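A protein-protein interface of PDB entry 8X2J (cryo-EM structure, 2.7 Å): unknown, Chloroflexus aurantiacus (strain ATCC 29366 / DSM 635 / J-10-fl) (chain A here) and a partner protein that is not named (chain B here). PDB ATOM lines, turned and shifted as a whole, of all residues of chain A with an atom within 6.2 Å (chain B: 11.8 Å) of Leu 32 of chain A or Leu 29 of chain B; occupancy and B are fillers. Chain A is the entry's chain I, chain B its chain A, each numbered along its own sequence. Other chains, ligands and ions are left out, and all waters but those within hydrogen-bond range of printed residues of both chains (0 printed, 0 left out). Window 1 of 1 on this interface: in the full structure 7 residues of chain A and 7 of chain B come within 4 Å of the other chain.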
ATOM      1  N   LEU A  27      25.904  38.868 -14.193  1.00  0.00           N
ATOM      2  CA  LEU A  27      27.305  38.457 -14.234  1.00  0.00           C
ATOM      3  C   LEU A  27      27.510  37.090 -13.600  1.00  0.00           C
ATOM      4  O   LEU A  27      28.332  36.303 -14.080  1.00  0.00           O
ATOM      5  CB  LEU A  27      28.183  39.491 -13.534  1.00  0.00           C
ATOM      6  CG  LEU A  27      28.566  40.732 -14.339  1.00  0.00           C
ATOM      7  CD1 LEU A  27      29.481  41.627 -13.522  1.00  0.00           C
ATOM      8  CD2 LEU A  27      29.221  40.338 -15.652  1.00  0.00           C
ATOM      9  N   LEU A  28      26.747  36.779 -12.554  1.00  0.00           N
ATOM     10  CA  LEU A  28      26.868  35.488 -11.893  1.00  0.00           C
ATOM     11  C   LEU A  28      26.308  34.362 -12.760  1.00  0.00           C
ATOM     12  O   LEU A  28      26.894  33.273 -12.828  1.00  0.00           O
ATOM     13  CB  LEU A  28      26.155  35.568 -10.548  1.00  0.00           C
ATOM     14  CG  LEU A  28      26.573  34.692  -9.386  1.00  0.00           C
ATOM     15  CD1 LEU A  28      28.055  34.832  -9.122  1.00  0.00           C
ATOM     16  CD2 LEU A  28      25.789  35.180  -8.205  1.00  0.00           C
ATOM     17  N   MET A  29      25.186  34.616 -13.448  1.00  0.00           N
ATOM     18  CA  MET A  29      24.640  33.637 -14.385  1.00  0.00           C
ATOM     19  C   MET A  29      25.568  33.434 -15.578  1.00  0.00           C
ATOM     20  O   MET A  29      25.727  32.307 -16.060  1.00  0.00           O
ATOM     21  CB  MET A  29      23.254  34.075 -14.860  1.00  0.00           C
ATOM     22  CG  MET A  29      22.149  33.953 -13.821  1.00  0.00           C
ATOM     23  SD  MET A  29      21.346  32.347 -13.780  1.00  0.00           S
ATOM     24  CE  MET A  29      22.039  31.689 -12.271  1.00  0.00           C
ATOM     25  N   VAL A  30      26.188  34.518 -16.063  1.00  0.00           N
ATOM     26  CA  VAL A  30      27.159  34.421 -17.154  1.00  0.00           C
ATOM     27  C   VAL A  30      28.379  33.617 -16.720  1.00  0.00           C
ATOM     28  O   VAL A  30      28.872  32.770 -17.474  1.00  0.00           O
ATOM     29  CB  VAL A  30      27.533  35.833 -17.656  1.00  0.00           C
ATOM     30  CG1 VAL A  30      28.802  35.820 -18.491  1.00  0.00           C
ATOM     31  CG2 VAL A  30      26.408  36.384 -18.505  1.00  0.00           C
ATOM     32  N   TRP A  31      28.851  33.834 -15.488  1.00  0.00           N
ATOM     33  CA  TRP A  31      29.980  33.069 -14.960  1.00  0.00           C
ATOM     34  C   TRP A  31      29.649  31.584 -14.850  1.00  0.00           C
ATOM     35  O   TRP A  31      30.423  30.736 -15.312  1.00  0.00           O
ATOM     36  CB  TRP A  31      30.395  33.639 -13.603  1.00  0.00           C
ATOM     37  CG  TRP A  31      31.585  32.978 -12.969  1.00  0.00           C
ATOM     38  CD1 TRP A  31      32.592  32.307 -13.598  1.00  0.00           C
ATOM     39  CD2 TRP A  31      31.906  32.964 -11.573  1.00  0.00           C
ATOM     40  NE1 TRP A  31      33.505  31.854 -12.679  1.00  0.00           N
ATOM     41  CE2 TRP A  31      33.109  32.248 -11.429  1.00  0.00           C
ATOM     42  CE3 TRP A  31      31.288  33.480 -10.431  1.00  0.00           C
ATOM     43  CZ2 TRP A  31      33.707  32.037 -10.190  1.00  0.00           C
ATOM     44  CZ3 TRP A  31      31.884  33.269  -9.200  1.00  0.00           C
ATOM     45  CH2 TRP A  31      33.081  32.554  -9.090  1.00  0.00           C
ATOM     46  N   LEU A  32      28.477  31.259 -14.294  1.00  0.00           N
ATOM     47  CA  LEU A  32      28.078  29.862 -14.132  1.00  0.00           C
ATOM     48  C   LEU A  32      27.841  29.173 -15.474  1.00  0.00           C
ATOM     49  O   LEU A  32      28.194  28.002 -15.646  1.00  0.00           O
ATOM     50  CB  LEU A  32      26.828  29.776 -13.252  1.00  0.00           C
ATOM     51  CG  LEU A  32      25.898  28.562 -13.371  1.00  0.00           C
ATOM     52  CD1 LEU A  32      26.541  27.299 -12.822  1.00  0.00           C
ATOM     53  CD2 LEU A  32      24.573  28.832 -12.682  1.00  0.00           C
ATOM     54  N   PHE A  33      27.263  29.870 -16.443  1.00  0.00           N
ATOM     55  CA  PHE A  33      26.873  29.218 -17.680  1.00  0.00           C
ATOM     56  C   PHE A  33      27.878  29.395 -18.810  1.00  0.00           C
ATOM     57  O   PHE A  33      27.675  28.830 -19.888  1.00  0.00           O
ATOM     58  CB  PHE A  33      25.497  29.722 -18.108  1.00  0.00           C
ATOM     59  CG  PHE A  33      24.389  29.248 -17.217  1.00  0.00           C
ATOM     60  CD1 PHE A  33      24.300  27.910 -16.861  1.00  0.00           C
ATOM     61  CD2 PHE A  33      23.444  30.132 -16.727  1.00  0.00           C
ATOM     62  CE1 PHE A  33      23.285  27.464 -16.041  1.00  0.00           C
ATOM     63  CE2 PHE A  33      22.427  29.692 -15.904  1.00  0.00           C
ATOM     64  CZ  PHE A  33      22.348  28.356 -15.561  1.00  0.00           C
ATOM     65  N   ALA A  34      28.948  30.147 -18.600  1.00  0.00           N
ATOM     66  CA  ALA A  34      29.946  30.289 -19.649  1.00  0.00           C
ATOM     67  C   ALA A  34      31.368  30.041 -19.176  1.00  0.00           C
ATOM     68  O   ALA A  34      32.165  29.487 -19.934  1.00  0.00           O
ATOM     69  CB  ALA A  34      29.845  31.687 -20.274  1.00  0.00           C
ATOM     70  N   PHE A  35      31.716  30.440 -17.949  1.00  0.00           N
ATOM     71  CA  PHE A  35      33.106  30.424 -17.510  1.00  0.00           C
ATOM     72  C   PHE A  35      33.305  29.530 -16.293  1.00  0.00           C
ATOM     73  O   PHE A  35      34.181  29.783 -15.464  1.00  0.00           O
ATOM     74  CB  PHE A  35      33.594  31.842 -17.217  1.00  0.00           C
ATOM     75  CG  PHE A  35      33.501  32.766 -18.397  1.00  0.00           C
ATOM     76  CD1 PHE A  35      34.488  32.766 -19.370  1.00  0.00           C
ATOM     77  CD2 PHE A  35      32.428  33.631 -18.534  1.00  0.00           C
ATOM     78  CE1 PHE A  35      34.404  33.613 -20.460  1.00  0.00           C
ATOM     79  CE2 PHE A  35      32.338  34.479 -19.622  1.00  0.00           C
ATOM     80  CZ  PHE A  35      33.328  34.470 -20.585  1.00  0.00           C
ATOM     81  N   TYR A  36      32.498  28.478 -16.176  1.00  0.00           N
ATOM     82  CA  TYR A  36      32.557  27.577 -15.034  1.00  0.00           C
ATOM     83  C   TYR A  36      33.183  26.236 -15.397  1.00  0.00           C
ATOM     84  O   TYR A  36      34.197  25.857 -14.803  1.00  0.00           O
ATOM     85  CB  TYR A  36      31.143  27.385 -14.481  1.00  0.00           C
ATOM     86  CG  TYR A  36      31.064  26.732 -13.129  1.00  0.00           C
ATOM     87  CD1 TYR A  36      31.934  27.092 -12.115  1.00  0.00           C
ATOM     88  CD2 TYR A  36      30.094  25.775 -12.860  1.00  0.00           C
ATOM     89  CE1 TYR A  36      31.859  26.498 -10.879  1.00  0.00           C
ATOM     90  CE2 TYR A  36      30.010  25.179 -11.622  1.00  0.00           C
ATOM     91  CZ  TYR A  36      30.893  25.549 -10.637  1.00  0.00           C
ATOM     92  OH  TYR A  36      30.814  24.962  -9.403  1.00  0.00           O
ATOM     93  N   TRP A  37      32.604  25.534 -16.376  1.00  0.00           N
ATOM     94  CA  TRP A  37      33.102  24.272 -16.943  1.00  0.00           C
ATOM     95  C   TRP A  37      33.372  23.176 -15.912  1.00  0.00           C
ATOM     96  O   TRP A  37      34.511  22.980 -15.489  1.00  0.00           O
ATOM     97  CB  TRP A  37      34.369  24.526 -17.768  1.00  0.00           C
ATOM     98  CG  TRP A  37      34.238  25.675 -18.717  1.00  0.00           C
ATOM     99  CD1 TRP A  37      33.196  25.928 -19.560  1.00  0.00           C
ATOM    100  CD2 TRP A  37      35.184  26.731 -18.923  1.00  0.00           C
ATOM    101  NE1 TRP A  37      33.432  27.075 -20.274  1.00  0.00           N
ATOM    102  CE2 TRP A  37      34.648  27.586 -19.904  1.00  0.00           C
ATOM    103  CE3 TRP A  37      36.432  27.035 -18.371  1.00  0.00           C
ATOM    104  CZ2 TRP A  37      35.316  28.728 -20.346  1.00  0.00           C
ATOM    105  CZ3 TRP A  37      37.094  28.168 -18.811  1.00  0.00           C
ATOM    106  CH2 TRP A  37      36.535  29.000 -19.789  1.00  0.00           C
ATOM    107  N   LEU B  20      11.780  36.845  -3.351  1.00  0.00           N
ATOM    108  CA  LEU B  20      11.271  35.804  -4.240  1.00  0.00           C
ATOM    109  C   LEU B  20      12.053  35.756  -5.547  1.00  0.00           C
ATOM    110  O   LEU B  20      12.373  34.666  -6.044  1.00  0.00           O
ATOM    111  CB  LEU B  20       9.784  36.031  -4.511  1.00  0.00           C
ATOM    112  CG  LEU B  20       9.054  34.927  -5.276  1.00  0.00           C
ATOM    113  CD1 LEU B  20       8.898  33.689  -4.410  1.00  0.00           C
ATOM    114  CD2 LEU B  20       7.704  35.418  -5.768  1.00  0.00           C
ATOM    115  N   VAL B  21      12.383  36.925  -6.108  1.00  0.00           N
ATOM    116  CA  VAL B  21      13.201  36.966  -7.323  1.00  0.00           C
ATOM    117  C   VAL B  21      14.605  36.429  -7.046  1.00  0.00           C
ATOM    118  O   VAL B  21      15.144  35.622  -7.820  1.00  0.00           O
ATOM    119  CB  VAL B  21      13.229  38.397  -7.895  1.00  0.00           C
ATOM    120  CG1 VAL B  21      14.252  38.527  -9.015  1.00  0.00           C
ATOM    121  CG2 VAL B  21      11.851  38.784  -8.402  1.00  0.00           C
ATOM    122  N   LEU B  22      15.197  36.829  -5.912  1.00  0.00           N
ATOM    123  CA  LEU B  22      16.510  36.322  -5.520  1.00  0.00           C
ATOM    124  C   LEU B  22      16.485  34.826  -5.228  1.00  0.00           C
ATOM    125  O   LEU B  22      17.465  34.132  -5.502  1.00  0.00           O
ATOM    126  CB  LEU B  22      17.025  37.079  -4.298  1.00  0.00           C
ATOM    127  CG  LEU B  22      17.608  38.473  -4.522  1.00  0.00           C
ATOM    128  CD1 LEU B  22      18.256  38.974  -3.248  1.00  0.00           C
ATOM    129  CD2 LEU B  22      18.608  38.465  -5.659  1.00  0.00           C
ATOM    130  N   LEU B  23      15.370  34.313  -4.706  1.00  0.00           N
ATOM    131  CA  LEU B  23      15.258  32.888  -4.418  1.00  0.00           C
ATOM    132  C   LEU B  23      15.124  32.075  -5.697  1.00  0.00           C
ATOM    133  O   LEU B  23      15.666  30.968  -5.789  1.00  0.00           O
ATOM    134  CB  LEU B  23      14.066  32.646  -3.493  1.00  0.00           C
ATOM    135  CG  LEU B  23      14.148  31.460  -2.536  1.00  0.00           C
ATOM    136  CD1 LEU B  23      15.125  31.757  -1.412  1.00  0.00           C
ATOM    137  CD2 LEU B  23      12.771  31.136  -1.983  1.00  0.00           C
ATOM    138  N   VAL B  24      14.410  32.609  -6.694  1.00  0.00           N
ATOM    139  CA  VAL B  24      14.323  31.947  -7.999  1.00  0.00           C
ATOM    140  C   VAL B  24      15.693  31.905  -8.673  1.00  0.00           C
ATOM    141  O   VAL B  24      16.110  30.863  -9.210  1.00  0.00           O
ATOM    142  CB  VAL B  24      13.268  32.653  -8.874  1.00  0.00           C
ATOM    143  CG1 VAL B  24      13.407  32.266 -10.338  1.00  0.00           C
ATOM    144  CG2 VAL B  24      11.872  32.331  -8.373  1.00  0.00           C
ATOM    145  N   VAL B  25      16.426  33.024  -8.618  1.00  0.00           N
ATOM    146  CA  VAL B  25      17.770  33.086  -9.198  1.00  0.00           C
ATOM    147  C   VAL B  25      18.723  32.145  -8.463  1.00  0.00           C
ATOM    148  O   VAL B  25      19.521  31.434  -9.089  1.00  0.00           O
ATOM    149  CB  VAL B  25      18.274  34.544  -9.198  1.00  0.00           C
ATOM    150  CG1 VAL B  25      19.755  34.629  -9.536  1.00  0.00           C
ATOM    151  CG2 VAL B  25      17.470  35.373 -10.185  1.00  0.00           C
ATOM    152  N   GLU B  26      18.615  32.081  -7.132  1.00  0.00           N
ATOM    153  CA  GLU B  26      19.464  31.195  -6.340  1.00  0.00           C
ATOM    154  C   GLU B  26      19.136  29.726  -6.585  1.00  0.00           C
ATOM    155  O   GLU B  26      20.035  28.883  -6.577  1.00  0.00           O
ATOM    156  CB  GLU B  26      19.322  31.534  -4.856  1.00  0.00           C
ATOM    157  CG  GLU B  26      20.323  30.844  -3.951  1.00  0.00           C
ATOM    158  CD  GLU B  26      21.755  31.174  -4.311  1.00  0.00           C
ATOM    159  OE1 GLU B  26      22.130  32.360  -4.225  1.00  0.00           O
ATOM    160  OE2 GLU B  26      22.511  30.247  -4.668  1.00  0.00           O
ATOM    161  N   GLY B  27      17.861  29.400  -6.805  1.00  0.00           N
ATOM    162  CA  GLY B  27      17.504  28.029  -7.135  1.00  0.00           C
ATOM    163  C   GLY B  27      18.024  27.591  -8.491  1.00  0.00           C
ATOM    164  O   GLY B  27      18.532  26.471  -8.636  1.00  0.00           O
ATOM    165  N   ILE B  28      17.913  28.469  -9.497  1.00  0.00           N
ATOM    166  CA  ILE B  28      18.472  28.184 -10.820  1.00  0.00           C
ATOM    167  C   ILE B  28      19.990  28.036 -10.738  1.00  0.00           C
ATOM    168  O   ILE B  28      20.579  27.127 -11.342  1.00  0.00           O
ATOM    169  CB  ILE B  28      18.053  29.287 -11.815  1.00  0.00           C
ATOM    170  CG1 ILE B  28      16.546  29.227 -12.067  1.00  0.00           C
ATOM    171  CG2 ILE B  28      18.809  29.176 -13.131  1.00  0.00           C
ATOM    172  CD1 ILE B  28      16.037  30.311 -12.989  1.00  0.00           C
ATOM    173  N   LEU B  29      20.630  28.896  -9.944  1.00  0.00           N
ATOM    174  CA  LEU B  29      22.072  28.832  -9.744  1.00  0.00           C
ATOM    175  C   LEU B  29      22.493  27.549  -9.037  1.00  0.00           C
ATOM    176  O   LEU B  29      23.498  26.939  -9.410  1.00  0.00           O
ATOM    177  CB  LEU B  29      22.520  30.060  -8.955  1.00  0.00           C
ATOM    178  CG  LEU B  29      24.002  30.363  -8.813  1.00  0.00           C
ATOM    179  CD1 LEU B  29      24.196  31.837  -9.032  1.00  0.00           C
ATOM    180  CD2 LEU B  29      24.470  29.983  -7.428  1.00  0.00           C
ATOM    181  N   ILE B  30      21.736  27.124  -8.021  1.00  0.00           N
ATOM    182  CA  ILE B  30      22.058  25.906  -7.280  1.00  0.00           C
ATOM    183  C   ILE B  30      21.908  24.680  -8.174  1.00  0.00           C
ATOM    184  O   ILE B  30      22.752  23.776  -8.151  1.00  0.00           O
ATOM    185  CB  ILE B  30      21.184  25.823  -6.011  1.00  0.00           C
ATOM    186  CG1 ILE B  30      21.819  26.628  -4.876  1.00  0.00           C
ATOM    187  CG2 ILE B  30      20.955  24.386  -5.550  1.00  0.00           C
ATOM    188  CD1 ILE B  30      20.943  26.746  -3.652  1.00  0.00           C
ATOM    189  N   LEU B  31      20.863  24.657  -9.010  1.00  0.00           N
ATOM    190  CA  LEU B  31      20.681  23.559  -9.957  1.00  0.00           C
ATOM    191  C   LEU B  31      21.811  23.505 -10.985  1.00  0.00           C
ATOM    192  O   LEU B  31      22.331  22.421 -11.288  1.00  0.00           O
ATOM    193  CB  LEU B  31      19.325  23.694 -10.647  1.00  0.00           C
ATOM    194  CG  LEU B  31      18.900  22.591 -11.612  1.00  0.00           C
ATOM    195  CD1 LEU B  31      18.861  21.249 -10.908  1.00  0.00           C
ATOM    196  CD2 LEU B  31      17.548  22.921 -12.205  1.00  0.00           C
ATOM    197  N   GLY B  32      22.224  24.666 -11.507  1.00  0.00           N
ATOM    198  CA  GLY B  32      23.321  24.691 -12.465  1.00  0.00           C
ATOM    199  C   GLY B  32      24.657  24.286 -11.868  1.00  0.00           C
ATOM    200  O   GLY B  32      25.409  23.516 -12.476  1.00  0.00           O
ATOM    201  N   VAL B  33      24.962  24.785 -10.665  1.00  0.00           N
ATOM    202  CA  VAL B  33      26.200  24.424  -9.976  1.00  0.00           C
ATOM    203  C   VAL B  33      26.211  22.943  -9.616  1.00  0.00           C
ATOM    204  O   VAL B  33      27.246  22.276  -9.738  1.00  0.00           O
ATOM    205  CB  VAL B  33      26.404  25.332  -8.745  1.00  0.00           C
ATOM    206  CG1 VAL B  33      27.573  24.886  -7.928  1.00  0.00           C
ATOM    207  CG2 VAL B  33      26.698  26.742  -9.184  1.00  0.00           C
ATOM    208  N   TYR B  34      25.063  22.386  -9.214  1.00  0.00           N
ATOM    209  CA  TYR B  34      25.019  20.955  -8.924  1.00  0.00           C
ATOM    210  C   TYR B  34      25.209  20.116 -10.182  1.00  0.00           C
ATOM    211  O   TYR B  34      25.898  19.094 -10.146  1.00  0.00           O
ATOM    212  CB  TYR B  34      23.712  20.564  -8.242  1.00  0.00           C
ATOM    213  CG  TYR B  34      23.701  19.097  -7.877  1.00  0.00           C
ATOM    214  CD1 TYR B  34      24.500  18.622  -6.844  1.00  0.00           C
ATOM    215  CD2 TYR B  34      22.931  18.183  -8.587  1.00  0.00           C
ATOM    216  CE1 TYR B  34      24.513  17.284  -6.511  1.00  0.00           C
ATOM    217  CE2 TYR B  34      22.942  16.840  -8.263  1.00  0.00           C
ATOM    218  CZ  TYR B  34      23.735  16.401  -7.223  1.00  0.00           C
ATOM    219  OH  TYR B  34      23.752  15.071  -6.889  1.00  0.00           O
ATOM    220  N   PHE B  35      24.623  20.525 -11.304  1.00  0.00           N
ATOM    221  CA  PHE B  35      24.810  19.722 -12.504  1.00  0.00           C
ATOM    222  C   PHE B  35      26.159  19.949 -13.171  1.00  0.00           C
ATOM    223  O   PHE B  35      26.521  19.183 -14.071  1.00  0.00           O
ATOM    224  CB  PHE B  35      23.679  19.978 -13.496  1.00  0.00           C
ATOM    225  CG  PHE B  35      22.561  18.988 -13.386  1.00  0.00           C
ATOM    226  CD1 PHE B  35      21.686  19.036 -12.313  1.00  0.00           C
ATOM    227  CD2 PHE B  35      22.395  17.999 -14.340  1.00  0.00           C
ATOM    228  CE1 PHE B  35      20.659  18.125 -12.198  1.00  0.00           C
ATOM    229  CE2 PHE B  35      21.367  17.083 -14.232  1.00  0.00           C
ATOM    230  CZ  PHE B  35      20.499  17.147 -13.159  1.00  0.00           C
ATOM    231  N   ARG B  36      26.909  20.972 -12.764  1.00  0.00           N
ATOM    232  CA  ARG B  36      28.267  21.168 -13.253  1.00  0.00           C
ATOM    233  C   ARG B  36      29.341  20.841 -12.223  1.00  0.00           C
ATOM    234  O   ARG B  36      30.528  21.008 -12.518  1.00  0.00           O
ATOM    235  CB  ARG B  36      28.444  22.611 -13.734  1.00  0.00           C
ATOM    236  CG  ARG B  36      27.731  22.913 -15.033  1.00  0.00           C
ATOM    237  CD  ARG B  36      27.270  24.353 -15.082  1.00  0.00           C
ATOM    238  NE  ARG B  36      27.018  24.812 -16.441  1.00  0.00           N
ATOM    239  CZ  ARG B  36      25.878  24.631 -17.092  1.00  0.00           C
ATOM    240  NH1 ARG B  36      24.867  23.978 -16.546  1.00  0.00           N
ATOM    241  NH2 ARG B  36      25.752  25.115 -18.324  1.00  0.00           N
ATOM    242  N   SER B  37      28.964  20.390 -11.029  1.00  0.00           N
ATOM    243  CA  SER B  37      29.913  20.217  -9.940  1.00  0.00           C
ATOM    244  C   SER B  37      30.824  19.009 -10.140  1.00  0.00           C
ATOM    245  O   SER B  37      30.494  18.037 -10.831  1.00  0.00           O
ATOM    246  CB  SER B  37      29.173  20.083  -8.610  1.00  0.00           C
ATOM    247  OG  SER B  37      28.245  19.017  -8.646  1.00  0.00           O
ATOM    248  N   ASN B  38      31.992  19.090  -9.496  1.00  0.00           N
ATOM    249  CA  ASN B  38      32.990  18.029  -9.562  1.00  0.00           C
ATOM    250  C   ASN B  38      32.532  16.770  -8.844  1.00  0.00           C
ATOM    251  O   ASN B  38      32.959  15.671  -9.206  1.00  0.00           O
ATOM    252  CB  ASN B  38      34.309  18.517  -8.966  1.00  0.00           C
ATOM    253  CG  ASN B  38      35.000  19.538  -9.838  1.00  0.00           C
ATOM    254  OD1 ASN B  38      34.499  19.904 -10.898  1.00  0.00           O
ATOM    255  ND2 ASN B  38      36.158  20.006  -9.394  1.00  0.00           N
ATOM    256  N   PHE B  40      29.297  15.721  -8.763  1.00  0.00           N
ATOM    257  CA  PHE B  40      28.334  15.119  -9.677  1.00  0.00           C
ATOM    258  C   PHE B  40      29.026  14.507 -10.884  1.00  0.00           C
ATOM    259  O   PHE B  40      28.660  13.414 -11.327  1.00  0.00           O
ATOM    260  CB  PHE B  40      27.321  16.175 -10.111  1.00  0.00           C
ATOM    261  CG  PHE B  40      26.226  15.661 -11.000  1.00  0.00           C
ATOM    262  CD1 PHE B  40      25.219  14.859 -10.493  1.00  0.00           C
ATOM    263  CD2 PHE B  40      26.180  16.020 -12.336  1.00  0.00           C
ATOM    264  CE1 PHE B  40      24.200  14.402 -11.311  1.00  0.00           C
ATOM    265  CE2 PHE B  40      25.164  15.568 -13.158  1.00  0.00           C
ATOM    266  CZ  PHE B  40      24.174  14.759 -12.643  1.00  0.00           C
ATOM    267  N   ARG B  41      30.040  15.181 -11.415  1.00  0.00           N
ATOM    268  CA  ARG B  41      30.722  14.699 -12.605  1.00  0.00           C
ATOM    269  C   ARG B  41      31.937  13.834 -12.291  1.00  0.00           C
ATOM    270  O   ARG B  41      32.615  13.399 -13.230  1.00  0.00           O
ATOM    271  CB  ARG B  41      31.128  15.887 -13.480  1.00  0.00           C
ATOM    272  CG  ARG B  41      29.963  16.742 -13.943  1.00  0.00           C
ATOM    273  CD  ARG B  41      28.957  15.924 -14.719  1.00  0.00           C
ATOM    274  NE  ARG B  41      29.591  15.157 -15.783  1.00  0.00           N
ATOM    275  CZ  ARG B  41      29.204  15.167 -17.049  1.00  0.00           C
ATOM    276  NH1 ARG B  41      28.175  15.893 -17.450  1.00  0.00           N
ATOM    277  NH2 ARG B  41      29.863  14.427 -17.932  1.00  0.00           N
ATOM    278  N   TYR B 160      32.469  16.903 -21.007  1.00  0.00           N
ATOM    279  CA  TYR B 160      31.308  17.596 -21.532  1.00  0.00           C
ATOM    280  C   TYR B 160      31.308  17.548 -23.052  1.00  0.00           C
ATOM    281  O   TYR B 160      32.363  17.494 -23.696  1.00  0.00           O
ATOM    282  CB  TYR B 160      31.300  19.054 -21.077  1.00  0.00           C
ATOM    283  CG  TYR B 160      31.050  19.272 -19.607  1.00  0.00           C
ATOM    284  CD1 TYR B 160      30.094  18.534 -18.924  1.00  0.00           C
ATOM    285  CD2 TYR B 160      31.769  20.224 -18.901  1.00  0.00           C
ATOM    286  CE1 TYR B 160      29.862  18.743 -17.579  1.00  0.00           C
ATOM    287  CE2 TYR B 160      31.547  20.435 -17.555  1.00  0.00           C
ATOM    288  CZ  TYR B 160      30.591  19.694 -16.902  1.00  0.00           C
ATOM    289  OH  TYR B 160      30.374  19.902 -15.566  1.00  0.00           O
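Of the 11 printed residues of chain A, 6 touch a printed residue of chain B.
Hydrophobic or aromatic side chains of chain A that line the printed part of chain B: Leu 28, Met 29, Leu 32, Phe 33 and Tyr 36.
Printed residues of chain B that touch a printed residue of chain A: Leu 29, Gly 32, Val 33, Arg 36 and Tyr 160.
Hydrophobic or aromatic side chains of chain B within 4 Å of the printed part of chain A: Leu 29, Val 33 and Tyr 160.
Among the printed residues, 10 pairs touch across the chains.
The backbone carbonyl oxygen of Trp 31 of chain A is in hydrogen-bond range of the backbone NH of Tyr 36 of chain A, at 3.2 Å.
OH of Tyr 160 of chain B is in hydrogen-bond range of O of Arg 36 of chain B, 3.2 Å away.
The backbone carbonyl oxygen of Ala 34 of chain A sits at hydrogen-bond distance from the indole nitrogen of Trp 37 of chain A (2.7 Å).
Leu 32 of chain A touches four residues of chain B.
Leu 29 of chain B touches just these residues of chain A: Leu 28 (3.7 Å), Met 29 (3.7 Å) and Leu 32 (3.9 Å).
Of chain B, only Leu 29 comes within 4 Å of Met 29 of chain A.
No residue of chain B comes within 4 Å of Val 30 of chain A.
No residue of chain B comes within 4 Å of Ala 34 of chain A.
Of the printed residues of chain A, Gly 32 of chain B touches Leu 32.
Printed residues of chain B within 4 Å of Trp 37 of chain A: Tyr 160.
Arg 41 of chain B touches none of the printed residues of chain A.
The nearest printed residue of chain B that does not touch Trp 37 of chain A is Arg 36 of chain B (4.9 Å).
The backbone carbonyl oxygen of Leu 32 of chain A lies within hydrogen-bond range of the guanidinium group of Arg 36 of chain B (3.5 Å).
Among the printed residues, merely in contact across the chains: Phe 33 of chain A with Arg 36 of chain B, Tyr 36 of chain A with Val 33 of chain B, Leu 32 of chain A with Val 33 of chain B, Tyr 36 of chain A with Arg 36 of chain B, Leu 32 of chain A with Gly 32 of chain B, Trp 37 of chain A with Tyr 160 of chain B, Met 29 of chain A with Leu 29 of chain B, Leu 28 of chain A with Leu 29 of chain B and Leu 32 of chain A with Leu 29 of chain B.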
